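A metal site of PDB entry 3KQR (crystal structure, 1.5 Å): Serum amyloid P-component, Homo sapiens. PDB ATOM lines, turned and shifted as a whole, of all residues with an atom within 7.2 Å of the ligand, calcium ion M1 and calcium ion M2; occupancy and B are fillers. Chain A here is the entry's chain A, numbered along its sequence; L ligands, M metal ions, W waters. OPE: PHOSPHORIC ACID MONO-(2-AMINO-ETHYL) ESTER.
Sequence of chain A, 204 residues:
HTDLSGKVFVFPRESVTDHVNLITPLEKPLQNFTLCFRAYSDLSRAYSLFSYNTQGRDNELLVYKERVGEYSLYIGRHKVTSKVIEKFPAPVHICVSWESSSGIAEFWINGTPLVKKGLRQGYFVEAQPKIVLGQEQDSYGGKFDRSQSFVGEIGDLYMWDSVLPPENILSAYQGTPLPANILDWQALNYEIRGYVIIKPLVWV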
ATOM      1  N   ALA A  46       0.478  34.071  25.536  1.00  0.00           N
ATOM      2  CA  ALA A  46       1.828  33.692  25.906  1.00  0.00           C
ATOM      3  C   ALA A  46       2.812  34.331  24.923  1.00  0.00           C
ATOM      4  O   ALA A  46       2.478  34.571  23.740  1.00  0.00           O
ATOM      5  CB  ALA A  46       1.979  32.172  25.870  1.00  0.00           C
ATOM      6  N   TYR A  47       4.027  34.583  25.392  1.00  0.00           N
ATOM      7  CA  TYR A  47       5.062  35.081  24.526  1.00  0.00           C
ATOM      8  C   TYR A  47       6.451  34.810  25.083  1.00  0.00           C
ATOM      9  O   TYR A  47       6.644  34.662  26.306  1.00  0.00           O
ATOM     10  CB  TYR A  47       4.912  36.581  24.252  1.00  0.00           C
ATOM     11  CG  TYR A  47       4.760  37.462  25.477  1.00  0.00           C
ATOM     12  CD1 TYR A  47       5.871  37.958  26.147  1.00  0.00           C
ATOM     13  CD2 TYR A  47       3.496  37.855  25.927  1.00  0.00           C
ATOM     14  CE1 TYR A  47       5.715  38.828  27.222  1.00  0.00           C
ATOM     15  CE2 TYR A  47       3.320  38.682  27.029  1.00  0.00           C
ATOM     16  CZ  TYR A  47       4.430  39.182  27.662  1.00  0.00           C
ATOM     17  OH  TYR A  47       4.220  40.056  28.712  1.00  0.00           O
ATOM     18  N   SER A  48       7.430  34.738  24.182  1.00  0.00           N
ATOM     19  CA  SER A  48       8.815  34.611  24.531  1.00  0.00           C
ATOM     20  C   SER A  48       9.450  35.968  24.871  1.00  0.00           C
ATOM     21  O   SER A  48       9.272  36.941  24.133  1.00  0.00           O
ATOM     22  CB  SER A  48       9.582  33.998  23.366  1.00  0.00           C
ATOM     23  OG  SER A  48      10.955  33.917  23.661  1.00  0.00           O
ATOM     24  N   SER A  51      15.268  34.333  24.051  1.00  0.00           N
ATOM     25  CA  SER A  51      15.424  33.034  23.410  1.00  0.00           C
ATOM     26  C   SER A  51      16.893  32.797  23.076  1.00  0.00           C
ATOM     27  O   SER A  51      17.509  33.567  22.315  1.00  0.00           O
ATOM     28  CB  SER A  51      14.557  33.047  22.156  1.00  0.00           C
ATOM     29  OG  SER A  51      14.701  31.891  21.347  1.00  0.00           O
ATOM     30  N   ASN A  53      19.225  29.842  21.768  1.00  0.00           N
ATOM     31  CA  ASN A  53      19.267  28.516  21.166  1.00  0.00           C
ATOM     32  C   ASN A  53      20.711  28.246  20.772  1.00  0.00           C
ATOM     33  O   ASN A  53      21.507  29.162  20.586  1.00  0.00           O
ATOM     34  CB  ASN A  53      18.308  28.449  19.970  1.00  0.00           C
ATOM     35  CG  ASN A  53      16.934  27.946  20.348  1.00  0.00           C
ATOM     36  OD1 ASN A  53      16.568  27.900  21.535  1.00  0.00           O
ATOM     37  ND2 ASN A  53      16.154  27.547  19.340  1.00  0.00           N
ATOM     38  N   ASP A  58      17.100  23.333  20.828  1.00  0.00           N
ATOM     39  CA  ASP A  58      15.997  24.289  21.020  1.00  0.00           C
ATOM     40  C   ASP A  58      15.828  24.550  22.524  1.00  0.00           C
ATOM     41  O   ASP A  58      16.081  23.663  23.360  1.00  0.00           O
ATOM     42  CB  ASP A  58      14.669  23.724  20.468  1.00  0.00           C
ATOM     43  CG  ASP A  58      13.539  24.767  20.397  1.00  0.00           C
ATOM     44  OD1 ASP A  58      13.858  25.943  20.178  1.00  0.00           O
ATOM     45  OD2 ASP A  58      12.341  24.417  20.541  1.00  0.00           O
ATOM     46  N   ASN A  59      15.331  25.746  22.844  1.00  0.00           N
ATOM     47  CA  ASN A  59      15.007  26.135  24.215  1.00  0.00           C
ATOM     48  C   ASN A  59      16.183  25.899  25.143  1.00  0.00           C
ATOM     49  O   ASN A  59      16.000  25.333  26.228  1.00  0.00           O
ATOM     50  CB  ASN A  59      13.725  25.419  24.683  1.00  0.00           C
ATOM     51  CG  ASN A  59      12.516  25.757  23.795  1.00  0.00           C
ATOM     52  OD1 ASN A  59      12.608  26.632  22.933  1.00  0.00           O
ATOM     53  ND2 ASN A  59      11.406  25.094  24.016  1.00  0.00           N
ATOM     54  N   GLU A  60      17.398  26.254  24.701  1.00  0.00           N
ATOM     55  CA  GLU A  60      18.570  25.941  25.528  1.00  0.00           C
ATOM     56  C   GLU A  60      18.521  26.805  26.768  1.00  0.00           C
ATOM     57  O   GLU A  60      18.779  26.329  27.874  1.00  0.00           O
ATOM     58  CB  GLU A  60      19.918  26.040  24.791  1.00  0.00           C
ATOM     59  CG  GLU A  60      21.146  25.737  25.629  1.00  0.00           C
ATOM     60  CD  GLU A  60      21.304  24.264  25.985  1.00  0.00           C
ATOM     61  OE1 GLU A  60      20.451  23.446  25.542  1.00  0.00           O
ATOM     62  OE2 GLU A  60      22.291  23.975  26.662  1.00  0.00           O
ATOM     63  N   LEU A  62      15.552  29.712  27.797  1.00  0.00           N
ATOM     64  CA  LEU A  62      14.402  30.459  27.317  1.00  0.00           C
ATOM     65  C   LEU A  62      13.638  31.042  28.494  1.00  0.00           C
ATOM     66  O   LEU A  62      13.298  30.314  29.446  1.00  0.00           O
ATOM     67  CB  LEU A  62      13.467  29.536  26.507  1.00  0.00           C
ATOM     68  CG  LEU A  62      12.104  30.078  26.099  1.00  0.00           C
ATOM     69  CD1 LEU A  62      12.182  31.265  25.147  1.00  0.00           C
ATOM     70  CD2 LEU A  62      11.234  29.005  25.452  1.00  0.00           C
ATOM     71  N   TYR A  64      10.092  32.738  29.283  1.00  0.00           N
ATOM     72  CA  TYR A  64       8.808  32.680  28.594  1.00  0.00           C
ATOM     73  C   TYR A  64       7.695  33.093  29.540  1.00  0.00           C
ATOM     74  O   TYR A  64       7.682  32.700  30.687  1.00  0.00           O
ATOM     75  CB  TYR A  64       8.558  31.224  28.134  1.00  0.00           C
ATOM     76  CG  TYR A  64       7.452  31.048  27.104  1.00  0.00           C
ATOM     77  CD1 TYR A  64       7.681  31.382  25.772  1.00  0.00           C
ATOM     78  CD2 TYR A  64       6.220  30.530  27.446  1.00  0.00           C
ATOM     79  CE1 TYR A  64       6.711  31.211  24.822  1.00  0.00           C
ATOM     80  CE2 TYR A  64       5.230  30.335  26.471  1.00  0.00           C
ATOM     81  CZ  TYR A  64       5.506  30.691  25.176  1.00  0.00           C
ATOM     82  OH  TYR A  64       4.545  30.535  24.171  1.00  0.00           O
ATOM     83  N   GLU A  66       3.954  32.665  30.269  1.00  0.00           N
ATOM     84  CA  GLU A  66       2.844  31.759  29.981  1.00  0.00           C
ATOM     85  C   GLU A  66       1.487  32.489  29.920  1.00  0.00           C
ATOM     86  O   GLU A  66       0.642  32.295  29.021  1.00  0.00           O
ATOM     87  CB  GLU A  66       2.776  30.738  31.134  1.00  0.00           C
ATOM     88  CG  GLU A  66       4.084  29.989  31.452  1.00  0.00           C
ATOM     89  CD  GLU A  66       4.444  28.965  30.363  1.00  0.00           C
ATOM     90  OE1 GLU A  66       3.609  28.788  29.440  1.00  0.00           O
ATOM     91  OE2 GLU A  66       5.553  28.344  30.436  1.00  0.00           O
ATOM     92  N   SER A  72       8.274  31.528  33.258  1.00  0.00           N
ATOM     93  CA  SER A  72       8.977  30.270  33.094  1.00  0.00           C
ATOM     94  C   SER A  72      10.393  30.440  32.607  1.00  0.00           C
ATOM     95  O   SER A  72      10.692  31.320  31.799  1.00  0.00           O
ATOM     96  CB  SER A  72       8.250  29.376  32.099  1.00  0.00           C
ATOM     97  OG  SER A  72       6.932  29.080  32.566  1.00  0.00           O
ATOM     98  N   TYR A  74      13.276  27.918  30.849  1.00  0.00           N
ATOM     99  CA  TYR A  74      13.728  26.646  30.315  1.00  0.00           C
ATOM    100  C   TYR A  74      15.231  26.600  30.303  1.00  0.00           C
ATOM    101  O   TYR A  74      15.895  27.575  29.920  1.00  0.00           O
ATOM    102  CB  TYR A  74      13.253  26.469  28.880  1.00  0.00           C
ATOM    103  CG  TYR A  74      11.773  26.326  28.685  1.00  0.00           C
ATOM    104  CD1 TYR A  74      10.922  27.376  28.852  1.00  0.00           C
ATOM    105  CD2 TYR A  74      11.240  25.112  28.264  1.00  0.00           C
ATOM    106  CE1 TYR A  74       9.555  27.240  28.640  1.00  0.00           C
ATOM    107  CE2 TYR A  74       9.890  24.969  28.045  1.00  0.00           C
ATOM    108  CZ  TYR A  74       9.049  26.024  28.232  1.00  0.00           C
ATOM    109  OH  TYR A  74       7.694  25.881  27.999  1.00  0.00           O
ATOM    110  N   ARG A  77      15.664  22.478  27.582  1.00  0.00           N
ATOM    111  CA  ARG A  77      14.364  21.875  27.326  1.00  0.00           C
ATOM    112  C   ARG A  77      13.539  21.507  28.561  1.00  0.00           C
ATOM    113  O   ARG A  77      12.357  21.235  28.448  1.00  0.00           O
ATOM    114  CB  ARG A  77      14.526  20.627  26.430  1.00  0.00           C
ATOM    115  CG  ARG A  77      14.895  21.005  25.020  1.00  0.00           C
ATOM    116  CD  ARG A  77      13.636  21.400  24.296  1.00  0.00           C
ATOM    117  NE  ARG A  77      12.784  20.248  24.060  1.00  0.00           N
ATOM    118  CZ  ARG A  77      12.681  19.636  22.888  1.00  0.00           C
ATOM    119  NH1 ARG A  77      13.381  20.079  21.845  1.00  0.00           N
ATOM    120  NH2 ARG A  77      11.883  18.587  22.767  1.00  0.00           N
ATOM    121  N   LYS A  79      11.844  22.767  32.191  1.00  0.00           N
ATOM    122  CA  LYS A  79      11.302  24.065  32.609  1.00  0.00           C
ATOM    123  C   LYS A  79      10.879  24.095  34.046  1.00  0.00           C
ATOM    124  O   LYS A  79      10.558  23.065  34.696  1.00  0.00           O
ATOM    125  CB  LYS A  79      10.151  24.533  31.722  1.00  0.00           C
ATOM    126  CG  LYS A  79       8.956  23.691  31.867  1.00  0.00           C
ATOM    127  CD  LYS A  79       7.841  24.115  30.912  1.00  0.00           C
ATOM    128  CE  LYS A  79       7.229  25.421  31.348  1.00  0.00           C
ATOM    129  NZ  LYS A  79       5.917  25.612  30.661  1.00  0.00           N
ATOM    130  N   GLU A 136      10.444  33.704  19.381  1.00  0.00           N
ATOM    131  CA  GLU A 136      10.883  32.466  19.958  1.00  0.00           C
ATOM    132  C   GLU A 136      11.499  31.583  18.861  1.00  0.00           C
ATOM    133  O   GLU A 136      10.863  31.332  17.848  1.00  0.00           O
ATOM    134  CB  GLU A 136       9.656  31.787  20.589  1.00  0.00           C
ATOM    135  CG  GLU A 136       9.988  30.918  21.736  1.00  0.00           C
ATOM    136  CD  GLU A 136      10.505  29.588  21.288  1.00  0.00           C
ATOM    137  OE1 GLU A 136       9.880  28.996  20.364  1.00  0.00           O
ATOM    138  OE2 GLU A 136      11.503  29.101  21.859  1.00  0.00           O
ATOM    139  N   GLN A 137      12.740  31.156  19.056  1.00  0.00           N
ATOM    140  CA  GLN A 137      13.412  30.343  18.056  1.00  0.00           C
ATOM    141  C   GLN A 137      12.972  28.917  18.184  1.00  0.00           C
ATOM    142  O   GLN A 137      12.870  28.405  19.296  1.00  0.00           O
ATOM    143  CB  GLN A 137      14.921  30.381  18.235  1.00  0.00           C
ATOM    144  CG  GLN A 137      15.561  31.735  18.048  1.00  0.00           C
ATOM    145  CD  GLN A 137      17.019  31.689  18.435  1.00  0.00           C
ATOM    146  OE1 GLN A 137      17.877  31.294  17.649  1.00  0.00           O
ATOM    147  NE2 GLN A 137      17.309  32.048  19.691  1.00  0.00           N
ATOM    148  N   ASP A 138      12.755  28.257  17.073  1.00  0.00           N
ATOM    149  CA  ASP A 138      12.629  26.801  17.087  1.00  0.00           C
ATOM    150  C   ASP A 138      13.812  26.170  16.336  1.00  0.00           C
ATOM    151  O   ASP A 138      13.983  24.945  16.348  1.00  0.00           O
ATOM    152  CB  ASP A 138      11.286  26.348  16.517  1.00  0.00           C
ATOM    153  CG  ASP A 138      10.152  26.483  17.515  1.00  0.00           C
ATOM    154  OD1 ASP A 138      10.455  26.643  18.731  1.00  0.00           O
ATOM    155  OD2 ASP A 138       8.952  26.425  17.134  1.00  0.00           O
ATOM    156  N   SER A 139      14.656  27.014  15.723  1.00  0.00           N
ATOM    157  CA  SER A 139      15.902  26.551  15.095  1.00  0.00           C
ATOM    158  C   SER A 139      17.093  27.381  15.591  1.00  0.00           C
ATOM    159  O   SER A 139      16.932  28.242  16.449  1.00  0.00           O
ATOM    160  CB  SER A 139      15.786  26.673  13.588  1.00  0.00           C
ATOM    161  OG  SER A 139      15.885  28.040  13.210  1.00  0.00           O
ATOM    162  N   GLY A 142      16.223  30.891  13.930  1.00  0.00           N
ATOM    163  CA  GLY A 142      14.999  31.078  13.174  1.00  0.00           C
ATOM    164  C   GLY A 142      13.838  30.192  13.581  1.00  0.00           C
ATOM    165  O   GLY A 142      13.689  29.842  14.749  1.00  0.00           O
ATOM    166  N   LYS A 143      13.000  29.843  12.604  1.00  0.00           N
ATOM    167  CA  LYS A 143      11.788  29.063  12.848  1.00  0.00           C
ATOM    168  C   LYS A 143      10.905  29.728  13.892  1.00  0.00           C
ATOM    169  O   LYS A 143      10.534  29.117  14.899  1.00  0.00           O
ATOM    170  CB  LYS A 143      12.122  27.634  13.309  1.00  0.00           C
ATOM    171  CG  LYS A 143      12.550  26.681  12.192  1.00  0.00           C
ATOM    172  CD  LYS A 143      11.372  25.860  11.692  1.00  0.00           C
ATOM    173  CE  LYS A 143      11.836  24.692  10.829  1.00  0.00           C
ATOM    174  NZ  LYS A 143      12.562  23.654  11.623  1.00  0.00           N
ATOM    175  N   PHE A 144      10.584  30.994  13.651  1.00  0.00           N
ATOM    176  CA  PHE A 144       9.717  31.761  14.530  1.00  0.00           C
ATOM    177  C   PHE A 144       8.241  31.371  14.416  1.00  0.00           C
ATOM    178  O   PHE A 144       7.821  30.681  13.504  1.00  0.00           O
ATOM    179  CB  PHE A 144       9.916  33.248  14.244  1.00  0.00           C
ATOM    180  CG  PHE A 144      11.371  33.692  14.270  1.00  0.00           C
ATOM    181  CD1 PHE A 144      12.256  33.177  15.211  1.00  0.00           C
ATOM    182  CD2 PHE A 144      11.839  34.634  13.375  1.00  0.00           C
ATOM    183  CE1 PHE A 144      13.585  33.605  15.258  1.00  0.00           C
ATOM    184  CE2 PHE A 144      13.158  35.063  13.396  1.00  0.00           C
ATOM    185  CZ  PHE A 144      14.043  34.548  14.337  1.00  0.00           C
ATOM    186  N   ASP A 145       7.455  31.829  15.377  1.00  0.00           N
ATOM    187  CA  ASP A 145       6.039  31.525  15.473  1.00  0.00           C
ATOM    188  C   ASP A 145       5.329  32.794  15.911  1.00  0.00           C
ATOM    189  O   ASP A 145       5.576  33.295  17.009  1.00  0.00           O
ATOM    190  CB  ASP A 145       5.837  30.411  16.503  1.00  0.00           C
ATOM    191  CG  ASP A 145       4.373  30.081  16.779  1.00  0.00           C
ATOM    192  OD1 ASP A 145       3.473  30.849  16.385  1.00  0.00           O
ATOM    193  OD2 ASP A 145       4.125  29.019  17.416  1.00  0.00           O
ATOM    194  N   GLN A 148       3.930  33.347  19.402  1.00  0.00           N
ATOM    195  CA  GLN A 148       4.849  33.495  20.549  1.00  0.00           C
ATOM    196  C   GLN A 148       5.671  34.777  20.466  1.00  0.00           C
ATOM    197  O   GLN A 148       6.558  35.017  21.299  1.00  0.00           O
ATOM    198  CB  GLN A 148       5.824  32.331  20.624  1.00  0.00           C
ATOM    199  CG  GLN A 148       5.118  31.011  20.634  1.00  0.00           C
ATOM    200  CD  GLN A 148       6.077  29.896  20.672  1.00  0.00           C
ATOM    201  OE1 GLN A 148       6.884  29.733  19.759  1.00  0.00           O
ATOM    202  NE2 GLN A 148       6.047  29.116  21.766  1.00  0.00           N
HETATM  203  CA  OPE L   1       8.424  27.065  24.177  1.00  0.00           C
HETATM  204  CB  OPE L   1       7.526  27.719  25.195  1.00  0.00           C
HETATM  205  O1  OPE L   1       7.440  26.469  20.494  1.00  0.00           O
HETATM  206  O2  OPE L   1       7.709  24.548  22.114  1.00  0.00           O
HETATM  207  O3  OPE L   1       9.685  26.049  21.677  1.00  0.00           O
HETATM  208  O4  OPE L   1       7.632  26.949  23.024  1.00  0.00           O
HETATM  209  N   OPE L   1       6.366  26.832  25.422  1.00  0.00           N
HETATM  210  P   OPE L   1       8.218  26.052  21.802  1.00  0.00           P
HETATM  211 CA    CA M   1       8.272  27.996  18.970  1.00  0.00          CA
HETATM  212 CA    CA M   2      11.622  26.988  20.756  1.00  0.00          CA
HETATM  213  O   HOH W   1       6.226  27.393  17.882  1.00  0.00           O
HETATM  214  O   HOH W   2       4.387  26.932  23.667  1.00  0.00           O
HETATM  215  O   HOH W   3       9.820  22.893  21.155  1.00  0.00           O
HETATM  216  O   HOH W   4       4.424  27.061  27.502  1.00  0.00           O
HETATM  217  O   HOH W   5       8.993  29.556  17.209  1.00  0.00           O
HETATM  218  O   HOH W   6       4.738  26.229  20.848  1.00  0.00           O
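Calcium ion M1 is bound by O1 of the ligand, 2.3 Å away.
The side-chain carboxylate (OE1) of Glu 136 binds calcium ion M1, 2.4 Å away.
Calcium ion M1 is bound by the side-chain amide oxygen (OE1) of Gln 148 (2.4 Å).
Calcium ion M1 is bound by water W1 (2.4 Å).
Water W5 is bound to calcium ion M1, 2.5 Å away.
Calcium ion M1 is bound by the side-chain carboxylate (OD2) of Asp 138 (2.5 Å).
OD1 of Asp 138 is bound to calcium ion M1, at 2.6 Å.
NE2 of Gln 148 lies within hydrogen-bond range of OH of Tyr 64, 3.2 Å away.
N of Asp 138 lies within hydrogen-bond range of O of Lys 143, at 3.2 Å.
NE2 of Gln 137 is in hydrogen-bond range of O of Ser 51 (3.0 Å).
OE1 of Gln 137 sits close to O of Ser 139 (3.4 Å).
O of Asn 59 is in hydrogen-bond range of N of Arg 77.
The side-chain carboxylate of Asp 58 lies close to the side-chain amide nitrogen of Asn 53, at 2.9 Å.
The side-chain amino group (NZ) of Lys 79 lies within hydrogen-bond range of the side-chain hydroxyl (OH) of Tyr 74, at 3.2 Å.
O of Tyr 64 is in hydrogen-bond range of N of Ser 72, 2.9 Å away.
Within 4 Å of calcium ion M2: Asp 58, Asn 59, Glu 136, Gln 137 and Asp 138.
The nearest printed residue that does not touch calcium ion M2 is Asn 53 (4.8 Å).
Leu 62 touches the ligand (CD2 to CA, 3.6 Å).
Tyr 64 touches the ligand.
Of the 24 residues printed, 8 come within 4 Å of the ligand.
The nearest printed residue that does not touch the ligand is Gln 137 (4.6 Å).
Water W5 lies within hydrogen-bond range of the backbone carbonyl oxygen of Glu 136 (2.7 Å), the backbone carbonyl oxygen of Lys 143 (2.8 Å) and the backbone NH of Asp 145 (3.3 Å).
Water W2 lies within hydrogen-bond range of N of the ligand (2.6 Å) and NE2 of Gln 148 (3.3 Å).
Water W4 bridges OE1 of Glu 66 and N of the ligand.
Calcium ion M2 is bound by an oxygen (O3) of the ligand (2.3 Å), the side-chain carboxylate (OD1) of Asp 138 (2.4 Å), the side-chain carboxylate (OE2) of Glu 136 (2.4 Å), the backbone carbonyl oxygen (O) of Gln 137 (2.4 Å), the side-chain amide oxygen (OD1) of Asn 59 (2.4 Å), the side-chain carboxylate (OD1) of Asp 58 (2.5 Å), the side-chain carboxylate (OD2) of Asp 58 (2.7 Å) and the side-chain carboxylate (OE1) of Glu 136 (2.7 Å).
Calcium ion M2 has eight donor atoms within binding distance.
Of the 24 residues printed, 3 come within 4 Å of calcium ion M1.
The nearest printed residue that does not touch calcium ion M1 is Asp 145 (4.2 Å).
N of the ligand is in hydrogen-bond range of OH of Tyr 74 (3.1 Å).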
